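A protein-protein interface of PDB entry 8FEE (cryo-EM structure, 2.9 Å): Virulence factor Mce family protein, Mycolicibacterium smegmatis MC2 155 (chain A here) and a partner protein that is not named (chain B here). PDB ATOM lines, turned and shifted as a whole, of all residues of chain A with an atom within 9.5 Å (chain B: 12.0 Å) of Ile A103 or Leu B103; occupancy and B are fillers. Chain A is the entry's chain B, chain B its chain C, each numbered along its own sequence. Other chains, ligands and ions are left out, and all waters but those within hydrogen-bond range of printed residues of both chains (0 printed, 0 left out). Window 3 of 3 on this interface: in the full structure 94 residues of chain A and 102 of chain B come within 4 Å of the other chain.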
ATOM      1  N   GLY A  48     -25.257 -18.327   8.999  1.00  0.00           N
ATOM      2  CA  GLY A  48     -25.266 -19.764   9.165  1.00  0.00           C
ATOM      3  C   GLY A  48     -26.001 -20.553   8.109  1.00  0.00           C
ATOM      4  O   GLY A  48     -26.214 -21.756   8.300  1.00  0.00           O
ATOM      5  N   ARG A  50     -26.393 -22.805   4.948  1.00  0.00           N
ATOM      6  CA  ARG A  50     -25.512 -23.795   4.347  1.00  0.00           C
ATOM      7  C   ARG A  50     -26.053 -24.214   2.983  1.00  0.00           C
ATOM      8  O   ARG A  50     -27.028 -23.656   2.475  1.00  0.00           O
ATOM      9  CB  ARG A  50     -25.356 -25.010   5.262  1.00  0.00           C
ATOM     10  CG  ARG A  50     -24.525 -24.775   6.507  1.00  0.00           C
ATOM     11  CD  ARG A  50     -24.246 -26.081   7.250  1.00  0.00           C
ATOM     12  NE  ARG A  50     -25.458 -26.767   7.684  1.00  0.00           N
ATOM     13  CZ  ARG A  50     -26.013 -27.793   7.053  1.00  0.00           C
ATOM     14  NH1 ARG A  50     -25.493 -28.284   5.939  1.00  0.00           N
ATOM     15  NH2 ARG A  50     -27.119 -28.341   7.550  1.00  0.00           N
ATOM     16  N   GLN A  53     -29.889 -26.692   2.340  1.00  0.00           N
ATOM     17  CA  GLN A  53     -31.020 -26.270   3.147  1.00  0.00           C
ATOM     18  C   GLN A  53     -32.137 -25.747   2.251  1.00  0.00           C
ATOM     19  O   GLN A  53     -31.918 -25.357   1.102  1.00  0.00           O
ATOM     20  CB  GLN A  53     -30.591 -25.215   4.164  1.00  0.00           C
ATOM     21  CG  GLN A  53     -29.743 -25.788   5.285  1.00  0.00           C
ATOM     22  CD  GLN A  53     -29.361 -24.759   6.321  1.00  0.00           C
ATOM     23  OE1 GLN A  53     -29.676 -23.581   6.184  1.00  0.00           O
ATOM     24  NE2 GLN A  53     -28.676 -25.199   7.368  1.00  0.00           N
ATOM     25  N   TYR A  99     -34.944 -18.728  10.879  1.00  0.00           N
ATOM     26  CA  TYR A  99     -34.640 -19.856  11.746  1.00  0.00           C
ATOM     27  C   TYR A  99     -35.559 -21.026  11.430  1.00  0.00           C
ATOM     28  O   TYR A  99     -36.734 -20.844  11.103  1.00  0.00           O
ATOM     29  CB  TYR A  99     -34.812 -19.470  13.216  1.00  0.00           C
ATOM     30  CG  TYR A  99     -33.650 -18.749  13.856  1.00  0.00           C
ATOM     31  CD1 TYR A  99     -32.822 -17.917  13.119  1.00  0.00           C
ATOM     32  CD2 TYR A  99     -33.388 -18.901  15.209  1.00  0.00           C
ATOM     33  CE1 TYR A  99     -31.763 -17.259  13.715  1.00  0.00           C
ATOM     34  CE2 TYR A  99     -32.336 -18.250  15.811  1.00  0.00           C
ATOM     35  CZ  TYR A  99     -31.525 -17.430  15.061  1.00  0.00           C
ATOM     36  OH  TYR A  99     -30.473 -16.780  15.663  1.00  0.00           O
ATOM     37  N   GLN A 100     -35.019 -22.235  11.537  1.00  0.00           N
ATOM     38  CA  GLN A 100     -35.840 -23.435  11.534  1.00  0.00           C
ATOM     39  C   GLN A 100     -36.022 -24.010  12.928  1.00  0.00           C
ATOM     40  O   GLN A 100     -37.076 -24.583  13.222  1.00  0.00           O
ATOM     41  CB  GLN A 100     -35.228 -24.497  10.616  1.00  0.00           C
ATOM     42  CG  GLN A 100     -36.172 -25.626  10.263  1.00  0.00           C
ATOM     43  CD  GLN A 100     -35.585 -26.564   9.234  1.00  0.00           C
ATOM     44  OE1 GLN A 100     -35.659 -26.307   8.032  1.00  0.00           O
ATOM     45  NE2 GLN A 100     -34.992 -27.657   9.698  1.00  0.00           N
ATOM     46  N   ASP A 101     -35.021 -23.854  13.788  1.00  0.00           N
ATOM     47  CA  ASP A 101     -35.101 -24.264  15.183  1.00  0.00           C
ATOM     48  C   ASP A 101     -34.019 -23.522  15.956  1.00  0.00           C
ATOM     49  O   ASP A 101     -33.203 -22.796  15.382  1.00  0.00           O
ATOM     50  CB  ASP A 101     -34.941 -25.776  15.329  1.00  0.00           C
ATOM     51  CG  ASP A 101     -33.834 -26.331  14.459  1.00  0.00           C
ATOM     52  OD1 ASP A 101     -33.706 -25.884  13.303  1.00  0.00           O
ATOM     53  OD2 ASP A 101     -33.088 -27.214  14.927  1.00  0.00           O
ATOM     54  N   LEU A 102     -34.019 -23.714  17.271  1.00  0.00           N
ATOM     55  CA  LEU A 102     -33.048 -23.089  18.157  1.00  0.00           C
ATOM     56  C   LEU A 102     -31.746 -23.876  18.259  1.00  0.00           C
ATOM     57  O   LEU A 102     -31.008 -23.704  19.237  1.00  0.00           O
ATOM     58  CB  LEU A 102     -33.661 -22.896  19.546  1.00  0.00           C
ATOM     59  CG  LEU A 102     -35.001 -22.158  19.574  1.00  0.00           C
ATOM     60  CD1 LEU A 102     -35.525 -22.039  20.995  1.00  0.00           C
ATOM     61  CD2 LEU A 102     -34.877 -20.785  18.932  1.00  0.00           C
ATOM     62  N   ILE A 103     -31.447 -24.731  17.281  1.00  0.00           N
ATOM     63  CA  ILE A 103     -30.236 -25.545  17.294  1.00  0.00           C
ATOM     64  C   ILE A 103     -29.218 -24.952  16.328  1.00  0.00           C
ATOM     65  O   ILE A 103     -28.007 -25.015  16.569  1.00  0.00           O
ATOM     66  CB  ILE A 103     -30.559 -27.011  16.949  1.00  0.00           C
ATOM     67  CG1 ILE A 103     -31.510 -27.593  17.990  1.00  0.00           C
ATOM     68  CG2 ILE A 103     -29.296 -27.855  16.894  1.00  0.00           C
ATOM     69  CD1 ILE A 103     -30.997 -27.469  19.405  1.00  0.00           C
ATOM     70  N   GLY A 104     -29.695 -24.358  15.238  1.00  0.00           N
ATOM     71  CA  GLY A 104     -28.795 -23.714  14.302  1.00  0.00           C
ATOM     72  C   GLY A 104     -29.115 -23.935  12.839  1.00  0.00           C
ATOM     73  O   GLY A 104     -28.352 -23.508  11.968  1.00  0.00           O
ATOM     74  N   ASN A 105     -30.230 -24.597  12.550  1.00  0.00           N
ATOM     75  CA  ASN A 105     -30.642 -24.830  11.173  1.00  0.00           C
ATOM     76  C   ASN A 105     -31.471 -23.659  10.667  1.00  0.00           C
ATOM     77  O   ASN A 105     -32.331 -23.138  11.381  1.00  0.00           O
ATOM     78  CB  ASN A 105     -31.442 -26.128  11.058  1.00  0.00           C
ATOM     79  CG  ASN A 105     -30.740 -27.303  11.705  1.00  0.00           C
ATOM     80  OD1 ASN A 105     -29.514 -27.402  11.675  1.00  0.00           O
ATOM     81  ND2 ASN A 105     -31.516 -28.202  12.296  1.00  0.00           N
ATOM     82  N   ARG A 106     -31.204 -23.249   9.432  1.00  0.00           N
ATOM     83  CA  ARG A 106     -31.864 -22.113   8.809  1.00  0.00           C
ATOM     84  C   ARG A 106     -32.557 -22.562   7.531  1.00  0.00           C
ATOM     85  O   ARG A 106     -32.426 -23.708   7.094  1.00  0.00           O
ATOM     86  CB  ARG A 106     -30.864 -20.994   8.493  1.00  0.00           C
ATOM     87  CG  ARG A 106     -29.937 -20.627   9.634  1.00  0.00           C
ATOM     88  CD  ARG A 106     -30.608 -19.699  10.621  1.00  0.00           C
ATOM     89  NE  ARG A 106     -29.674 -19.236  11.639  1.00  0.00           N
ATOM     90  CZ  ARG A 106     -29.512 -19.810  12.822  1.00  0.00           C
ATOM     91  NH1 ARG A 106     -30.218 -20.868  13.179  1.00  0.00           N
ATOM     92  NH2 ARG A 106     -28.619 -19.307  13.670  1.00  0.00           N
ATOM     93  N   LEU A 136     -28.573 -13.708  17.126  1.00  0.00           N
ATOM     94  CA  LEU A 136     -28.847 -13.743  18.561  1.00  0.00           C
ATOM     95  C   LEU A 136     -27.798 -13.002  19.385  1.00  0.00           C
ATOM     96  O   LEU A 136     -28.130 -12.437  20.433  1.00  0.00           O
ATOM     97  CB  LEU A 136     -28.950 -15.196  19.028  1.00  0.00           C
ATOM     98  CG  LEU A 136     -29.166 -15.472  20.517  1.00  0.00           C
ATOM     99  CD1 LEU A 136     -30.578 -15.103  20.934  1.00  0.00           C
ATOM    100  CD2 LEU A 136     -28.868 -16.925  20.838  1.00  0.00           C
ATOM    101  N   GLY B  50     -14.361 -16.852  25.710  1.00  0.00           N
ATOM    102  CA  GLY B  50     -15.812 -16.770  25.724  1.00  0.00           C
ATOM    103  C   GLY B  50     -16.491 -18.106  25.522  1.00  0.00           C
ATOM    104  O   GLY B  50     -17.492 -18.189  24.800  1.00  0.00           O
ATOM    105  N   GLY B  51     -15.966 -19.161  26.142  1.00  0.00           N
ATOM    106  CA  GLY B  51     -16.542 -20.480  25.993  1.00  0.00           C
ATOM    107  C   GLY B  51     -16.253 -21.158  24.676  1.00  0.00           C
ATOM    108  O   GLY B  51     -16.866 -22.191  24.383  1.00  0.00           O
ATOM    109  N   LEU B  52     -15.351 -20.607  23.868  1.00  0.00           N
ATOM    110  CA  LEU B  52     -15.022 -21.203  22.582  1.00  0.00           C
ATOM    111  C   LEU B  52     -14.282 -22.522  22.774  1.00  0.00           C
ATOM    112  O   LEU B  52     -13.498 -22.692  23.712  1.00  0.00           O
ATOM    113  CB  LEU B  52     -14.165 -20.240  21.760  1.00  0.00           C
ATOM    114  CG  LEU B  52     -14.170 -20.366  20.238  1.00  0.00           C
ATOM    115  CD1 LEU B  52     -15.552 -20.113  19.681  1.00  0.00           C
ATOM    116  CD2 LEU B  52     -13.172 -19.404  19.631  1.00  0.00           C
ATOM    117  N   ASN B  53     -14.544 -23.463  21.874  1.00  0.00           N
ATOM    118  CA  ASN B  53     -13.928 -24.779  21.898  1.00  0.00           C
ATOM    119  C   ASN B  53     -13.230 -25.045  20.572  1.00  0.00           C
ATOM    120  O   ASN B  53     -13.519 -24.407  19.556  1.00  0.00           O
ATOM    121  CB  ASN B  53     -14.963 -25.878  22.171  1.00  0.00           C
ATOM    122  CG  ASN B  53     -15.505 -25.832  23.583  1.00  0.00           C
ATOM    123  OD1 ASN B  53     -14.780 -25.525  24.529  1.00  0.00           O
ATOM    124  ND2 ASN B  53     -16.788 -26.137  23.733  1.00  0.00           N
ATOM    125  N   ASP B  56     -14.932 -25.134  16.778  1.00  0.00           N
ATOM    126  CA  ASP B  56     -15.997 -24.164  16.573  1.00  0.00           C
ATOM    127  C   ASP B  56     -15.792 -23.412  15.263  1.00  0.00           C
ATOM    128  O   ASP B  56     -14.664 -23.175  14.825  1.00  0.00           O
ATOM    129  CB  ASP B  56     -16.065 -23.180  17.738  1.00  0.00           C
ATOM    130  CG  ASP B  56     -16.604 -23.813  19.003  1.00  0.00           C
ATOM    131  OD1 ASP B  56     -17.421 -24.752  18.900  1.00  0.00           O
ATOM    132  OD2 ASP B  56     -16.221 -23.367  20.103  1.00  0.00           O
ATOM    133  N   LYS B  57     -16.902 -23.044  14.637  1.00  0.00           N
ATOM    134  CA  LYS B  57     -16.858 -22.500  13.289  1.00  0.00           C
ATOM    135  C   LYS B  57     -16.305 -21.080  13.266  1.00  0.00           C
ATOM    136  O   LYS B  57     -16.468 -20.299  14.209  1.00  0.00           O
ATOM    137  CB  LYS B  57     -18.251 -22.519  12.667  1.00  0.00           C
ATOM    138  CG  LYS B  57     -18.857 -23.903  12.566  1.00  0.00           C
ATOM    139  CD  LYS B  57     -17.874 -24.877  11.942  1.00  0.00           C
ATOM    140  CE  LYS B  57     -18.413 -26.293  11.962  1.00  0.00           C
ATOM    141  NZ  LYS B  57     -17.413 -27.272  11.452  1.00  0.00           N
ATOM    142  N   ARG B  59     -16.606 -17.973  10.486  1.00  0.00           N
ATOM    143  CA  ARG B  59     -17.453 -17.614   9.362  1.00  0.00           C
ATOM    144  C   ARG B  59     -17.179 -16.181   8.941  1.00  0.00           C
ATOM    145  O   ARG B  59     -16.847 -15.327   9.766  1.00  0.00           O
ATOM    146  CB  ARG B  59     -18.942 -17.763   9.715  1.00  0.00           C
ATOM    147  CG  ARG B  59     -19.259 -18.971  10.574  1.00  0.00           C
ATOM    148  CD  ARG B  59     -20.735 -19.326  10.552  1.00  0.00           C
ATOM    149  NE  ARG B  59     -21.566 -18.317  11.195  1.00  0.00           N
ATOM    150  CZ  ARG B  59     -22.753 -18.564  11.731  1.00  0.00           C
ATOM    151  NH1 ARG B  59     -23.259 -19.786  11.752  1.00  0.00           N
ATOM    152  NH2 ARG B  59     -23.449 -17.563  12.261  1.00  0.00           N
ATOM    153  N   ASP B  64     -19.731 -20.342   6.584  1.00  0.00           N
ATOM    154  CA  ASP B  64     -18.570 -20.985   7.186  1.00  0.00           C
ATOM    155  C   ASP B  64     -17.352 -20.904   6.277  1.00  0.00           C
ATOM    156  O   ASP B  64     -17.444 -21.106   5.063  1.00  0.00           O
ATOM    157  CB  ASP B  64     -18.881 -22.451   7.487  1.00  0.00           C
ATOM    158  CG  ASP B  64     -19.894 -22.621   8.598  1.00  0.00           C
ATOM    159  OD1 ASP B  64     -19.610 -22.187   9.732  1.00  0.00           O
ATOM    160  OD2 ASP B  64     -20.976 -23.187   8.338  1.00  0.00           O
ATOM    161  N   ARG B  98     -18.833 -14.858  19.174  1.00  0.00           N
ATOM    162  CA  ARG B  98     -20.239 -14.580  19.404  1.00  0.00           C
ATOM    163  C   ARG B  98     -20.995 -15.860  19.723  1.00  0.00           C
ATOM    164  O   ARG B  98     -20.639 -16.950  19.266  1.00  0.00           O
ATOM    165  CB  ARG B  98     -20.876 -13.897  18.192  1.00  0.00           C
ATOM    166  CG  ARG B  98     -20.672 -14.620  16.884  1.00  0.00           C
ATOM    167  CD  ARG B  98     -21.403 -13.908  15.767  1.00  0.00           C
ATOM    168  NE  ARG B  98     -22.847 -14.062  15.879  1.00  0.00           N
ATOM    169  CZ  ARG B  98     -23.522 -15.108  15.425  1.00  0.00           C
ATOM    170  NH1 ARG B  98     -22.911 -16.122  14.838  1.00  0.00           N
ATOM    171  NH2 ARG B  98     -24.844 -15.140  15.570  1.00  0.00           N
ATOM    172  N   THR B  99     -22.055 -15.701  20.512  1.00  0.00           N
ATOM    173  CA  THR B  99     -22.971 -16.790  20.818  1.00  0.00           C
ATOM    174  C   THR B  99     -23.872 -17.050  19.618  1.00  0.00           C
ATOM    175  O   THR B  99     -24.494 -16.125  19.088  1.00  0.00           O
ATOM    176  CB  THR B  99     -23.813 -16.449  22.047  1.00  0.00           C
ATOM    177  OG1 THR B  99     -22.953 -16.069  23.127  1.00  0.00           O
ATOM    178  CG2 THR B  99     -24.645 -17.644  22.471  1.00  0.00           C
ATOM    179  N   ASP B 100     -23.945 -18.308  19.192  1.00  0.00           N
ATOM    180  CA  ASP B 100     -24.748 -18.648  18.025  1.00  0.00           C
ATOM    181  C   ASP B 100     -26.150 -19.102  18.408  1.00  0.00           C
ATOM    182  O   ASP B 100     -27.129 -18.690  17.777  1.00  0.00           O
ATOM    183  CB  ASP B 100     -24.050 -19.738  17.206  1.00  0.00           C
ATOM    184  CG  ASP B 100     -24.756 -20.031  15.896  1.00  0.00           C
ATOM    185  OD1 ASP B 100     -25.531 -19.174  15.424  1.00  0.00           O
ATOM    186  OD2 ASP B 100     -24.535 -21.125  15.337  1.00  0.00           O
ATOM    187  N   THR B 101     -26.269 -19.942  19.434  1.00  0.00           N
ATOM    188  CA  THR B 101     -27.545 -20.499  19.852  1.00  0.00           C
ATOM    189  C   THR B 101     -27.698 -20.347  21.359  1.00  0.00           C
ATOM    190  O   THR B 101     -26.723 -20.149  22.087  1.00  0.00           O
ATOM    191  CB  THR B 101     -27.677 -21.977  19.459  1.00  0.00           C
ATOM    192  OG1 THR B 101     -26.528 -22.701  19.917  1.00  0.00           O
ATOM    193  CG2 THR B 101     -27.793 -22.117  17.952  1.00  0.00           C
ATOM    194  N   ILE B 102     -28.949 -20.441  21.819  1.00  0.00           N
ATOM    195  CA  ILE B 102     -29.245 -20.249  23.235  1.00  0.00           C
ATOM    196  C   ILE B 102     -28.631 -21.339  24.104  1.00  0.00           C
ATOM    197  O   ILE B 102     -28.396 -21.112  25.296  1.00  0.00           O
ATOM    198  CB  ILE B 102     -30.766 -20.170  23.466  1.00  0.00           C
ATOM    199  CG1 ILE B 102     -31.429 -21.519  23.189  1.00  0.00           C
ATOM    200  CG2 ILE B 102     -31.383 -19.094  22.591  1.00  0.00           C
ATOM    201  CD1 ILE B 102     -32.901 -21.545  23.510  1.00  0.00           C
ATOM    202  N   LEU B 103     -28.361 -22.519  23.545  1.00  0.00           N
ATOM    203  CA  LEU B 103     -27.794 -23.610  24.326  1.00  0.00           C
ATOM    204  C   LEU B 103     -26.305 -23.439  24.594  1.00  0.00           C
ATOM    205  O   LEU B 103     -25.767 -24.148  25.451  1.00  0.00           O
ATOM    206  CB  LEU B 103     -28.045 -24.945  23.624  1.00  0.00           C
ATOM    207  CG  LEU B 103     -29.509 -25.384  23.567  1.00  0.00           C
ATOM    208  CD1 LEU B 103     -29.656 -26.672  22.781  1.00  0.00           C
ATOM    209  CD2 LEU B 103     -30.069 -25.544  24.969  1.00  0.00           C
ATOM    210  N   GLY B 104     -25.630 -22.533  23.892  1.00  0.00           N
ATOM    211  CA  GLY B 104     -24.269 -22.186  24.247  1.00  0.00           C
ATOM    212  C   GLY B 104     -23.213 -22.486  23.203  1.00  0.00           C
ATOM    213  O   GLY B 104     -22.051 -22.712  23.550  1.00  0.00           O
ATOM    214  N   ARG B 105     -23.590 -22.495  21.928  1.00  0.00           N
ATOM    215  CA  ARG B 105     -22.628 -22.704  20.854  1.00  0.00           C
ATOM    216  C   ARG B 105     -22.020 -21.371  20.438  1.00  0.00           C
ATOM    217  O   ARG B 105     -22.744 -20.419  20.128  1.00  0.00           O
ATOM    218  CB  ARG B 105     -23.289 -23.382  19.654  1.00  0.00           C
ATOM    219  CG  ARG B 105     -23.793 -24.789  19.931  1.00  0.00           C
ATOM    220  CD  ARG B 105     -22.705 -25.663  20.538  1.00  0.00           C
ATOM    221  NE  ARG B 105     -21.533 -25.769  19.677  1.00  0.00           N
ATOM    222  CZ  ARG B 105     -21.440 -26.578  18.631  1.00  0.00           C
ATOM    223  NH1 ARG B 105     -22.444 -27.359  18.268  1.00  0.00           N
ATOM    224  NH2 ARG B 105     -20.311 -26.600  17.926  1.00  0.00           N
ATOM    225  N   LYS B 106     -20.693 -21.309  20.434  1.00  0.00           N
ATOM    226  CA  LYS B 106     -19.950 -20.108  20.091  1.00  0.00           C
ATOM    227  C   LYS B 106     -19.333 -20.257  18.707  1.00  0.00           C
ATOM    228  O   LYS B 106     -19.065 -21.372  18.249  1.00  0.00           O
ATOM    229  CB  LYS B 106     -18.856 -19.826  21.124  1.00  0.00           C
ATOM    230  CG  LYS B 106     -19.344 -19.819  22.561  1.00  0.00           C
ATOM    231  CD  LYS B 106     -20.199 -18.601  22.850  1.00  0.00           C
ATOM    232  CE  LYS B 106     -20.824 -18.685  24.229  1.00  0.00           C
ATOM    233  NZ  LYS B 106     -19.794 -18.779  25.295  1.00  0.00           N
ATOM    234  N   ASN B 107     -19.110 -19.126  18.041  1.00  0.00           N
ATOM    235  CA  ASN B 107     -18.399 -19.145  16.770  1.00  0.00           C
ATOM    236  C   ASN B 107     -17.783 -17.778  16.518  1.00  0.00           C
ATOM    237  O   ASN B 107     -18.197 -16.773  17.100  1.00  0.00           O
ATOM    238  CB  ASN B 107     -19.322 -19.544  15.612  1.00  0.00           C
ATOM    239  CG  ASN B 107     -20.305 -18.454  15.248  1.00  0.00           C
ATOM    240  OD1 ASN B 107     -21.342 -18.298  15.888  1.00  0.00           O
ATOM    241  ND2 ASN B 107     -19.987 -17.697  14.206  1.00  0.00           N
ATOM    242  N   TYR B 133     -21.073 -10.792  24.917  1.00  0.00           N
ATOM    243  CA  TYR B 133     -21.787 -10.586  26.172  1.00  0.00           C
ATOM    244  C   TYR B 133     -22.543 -11.870  26.485  1.00  0.00           C
ATOM    245  O   TYR B 133     -23.498 -12.221  25.785  1.00  0.00           O
ATOM    246  CB  TYR B 133     -22.731  -9.391  26.072  1.00  0.00           C
ATOM    247  CG  TYR B 133     -23.389  -9.004  27.377  1.00  0.00           C
ATOM    248  CD1 TYR B 133     -22.632  -8.746  28.509  1.00  0.00           C
ATOM    249  CD2 TYR B 133     -24.768  -8.881  27.472  1.00  0.00           C
ATOM    250  CE1 TYR B 133     -23.229  -8.387  29.700  1.00  0.00           C
ATOM    251  CE2 TYR B 133     -25.374  -8.521  28.658  1.00  0.00           C
ATOM    252  CZ  TYR B 133     -24.599  -8.276  29.768  1.00  0.00           C
ATOM    253  OH  TYR B 133     -25.197  -7.915  30.953  1.00  0.00           O
ATOM    254  N   GLN B 134     -22.103 -12.576  27.523  1.00  0.00           N
ATOM    255  CA  GLN B 134     -22.648 -13.889  27.827  1.00  0.00           C
ATOM    256  C   GLN B 134     -24.102 -13.792  28.273  1.00  0.00           C
ATOM    257  O   GLN B 134     -24.522 -12.813  28.894  1.00  0.00           O
ATOM    258  CB  GLN B 134     -21.816 -14.565  28.915  1.00  0.00           C
ATOM    259  CG  GLN B 134     -20.315 -14.562  28.662  1.00  0.00           C
ATOM    260  CD  GLN B 134     -19.888 -15.513  27.558  1.00  0.00           C
ATOM    261  OE1 GLN B 134     -20.699 -16.252  27.001  1.00  0.00           O
ATOM    262  NE2 GLN B 134     -18.600 -15.498  27.238  1.00  0.00           N
ATOM    263  N   ILE B 135     -24.877 -14.826  27.936  1.00  0.00           N
ATOM    264  CA  ILE B 135     -26.272 -14.880  28.364  1.00  0.00           C
ATOM    265  C   ILE B 135     -26.364 -14.983  29.881  1.00  0.00           C
ATOM    266  O   ILE B 135     -27.226 -14.354  30.511  1.00  0.00           O
ATOM    267  CB  ILE B 135     -26.993 -16.049  27.667  1.00  0.00           C
ATOM    268  CG1 ILE B 135     -26.982 -15.848  26.151  1.00  0.00           C
ATOM    269  CG2 ILE B 135     -28.418 -16.164  28.160  1.00  0.00           C
ATOM    270  CD1 ILE B 135     -27.921 -16.766  25.399  1.00  0.00           C
ATOM    271  N   TYR B 136     -25.471 -15.764  30.498  1.00  0.00           N
ATOM    272  CA  TYR B 136     -25.474 -15.843  31.953  1.00  0.00           C
ATOM    273  C   TYR B 136     -25.044 -14.526  32.583  1.00  0.00           C
ATOM    274  O   TYR B 136     -25.524 -14.176  33.664  1.00  0.00           O
ATOM    275  CB  TYR B 136     -24.598 -17.002  32.443  1.00  0.00           C
ATOM    276  CG  TYR B 136     -23.113 -16.889  32.175  1.00  0.00           C
ATOM    277  CD1 TYR B 136     -22.270 -16.259  33.082  1.00  0.00           C
ATOM    278  CD2 TYR B 136     -22.545 -17.461  31.045  1.00  0.00           C
ATOM    279  CE1 TYR B 136     -20.912 -16.169  32.853  1.00  0.00           C
ATOM    280  CE2 TYR B 136     -21.186 -17.381  30.811  1.00  0.00           C
ATOM    281  CZ  TYR B 136     -20.375 -16.732  31.716  1.00  0.00           C
ATOM    282  OH  TYR B 136     -19.023 -16.645  31.487  1.00  0.00           O
ATOM    283  N   PHE B 139     -28.294 -12.468  32.505  1.00  0.00           N
ATOM    284  CA  PHE B 139     -29.194 -12.877  33.580  1.00  0.00           C
ATOM    285  C   PHE B 139     -28.680 -12.415  34.936  1.00  0.00           C
ATOM    286  O   PHE B 139     -29.457 -11.930  35.767  1.00  0.00           O
ATOM    287  CB  PHE B 139     -29.389 -14.392  33.574  1.00  0.00           C
ATOM    288  CG  PHE B 139     -30.400 -14.869  32.574  1.00  0.00           C
ATOM    289  CD1 PHE B 139     -31.737 -14.550  32.725  1.00  0.00           C
ATOM    290  CD2 PHE B 139     -30.022 -15.651  31.500  1.00  0.00           C
ATOM    291  CE1 PHE B 139     -32.675 -14.988  31.814  1.00  0.00           C
ATOM    292  CE2 PHE B 139     -30.958 -16.094  30.588  1.00  0.00           C
ATOM    293  CZ  PHE B 139     -32.285 -15.761  30.745  1.00  0.00           C
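The guanidinium group (NH2) of Arg A106 is in salt-bridge range of the side-chain carboxylate (OD1) of Asp B100 (3.6 Å).
Among the printed residues, pairs that only touch across the chains: Gly A48 with Arg B59 (3.3 Å), Leu A102 with Thr B101 (3.8 Å), Leu A102 with Ile B102 (3.7 Å), Ile A103 with Thr B101 (3.2 Å), Ile A103 with Leu B103 (3.7 Å), Leu A136 with Asp B100 (3.9 Å), Leu A136 with Thr B101 (3.7 Å) and Leu A136 with Ile B102 (3.7 Å).
Printed residues of chain B within 4 Å of Gly A48: Arg B59.
No residue of chain B comes within 4 Å of Asp A101.
Printed residues of chain B within 4 Å of Leu A102: Thr B101 (3.8 Å) and Ile B102 (3.7 Å).
Ile A103 touches two residues of chain B.
Of the printed residues of chain B, Arg A106 touches Asp B100.
Printed residues of chain B within 4 Å of Leu A136: Asp B100 (3.9 Å), Thr B101 (3.7 Å) and Ile B102 (3.7 Å).
Of the printed residues of chain A, Ile B102 touches Leu A102 and Leu A136.
Of chain A, only Ile A103 comes within 4 Å of Leu B103.
Gly B104 touches none of the printed residues of chain A.
The nearest printed residue of chain A that does not touch Asp B100 is Tyr A99 (4.4 Å).
Among the printed residues, Asp or Glu carboxylates within 4 Å of a Lys or Arg side-chain nitrogen of the other chain: Arg A106 with Asp B100.
The backbone carbonyl oxygen (O) of Arg A106 sits close to the side-chain amide oxygen (OE1) of Gln A53 (2.9 Å).
NH1 of Arg A106 sits close to O of Gly A104, 3.5 Å away.
The guanidinium group (NE) of Arg B59 sits close to the side-chain amide nitrogen (ND2) of Asn B107 (3.5 Å).
N of Asp B100 is in hydrogen-bond range of O of Arg B105, at 2.6 Å.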
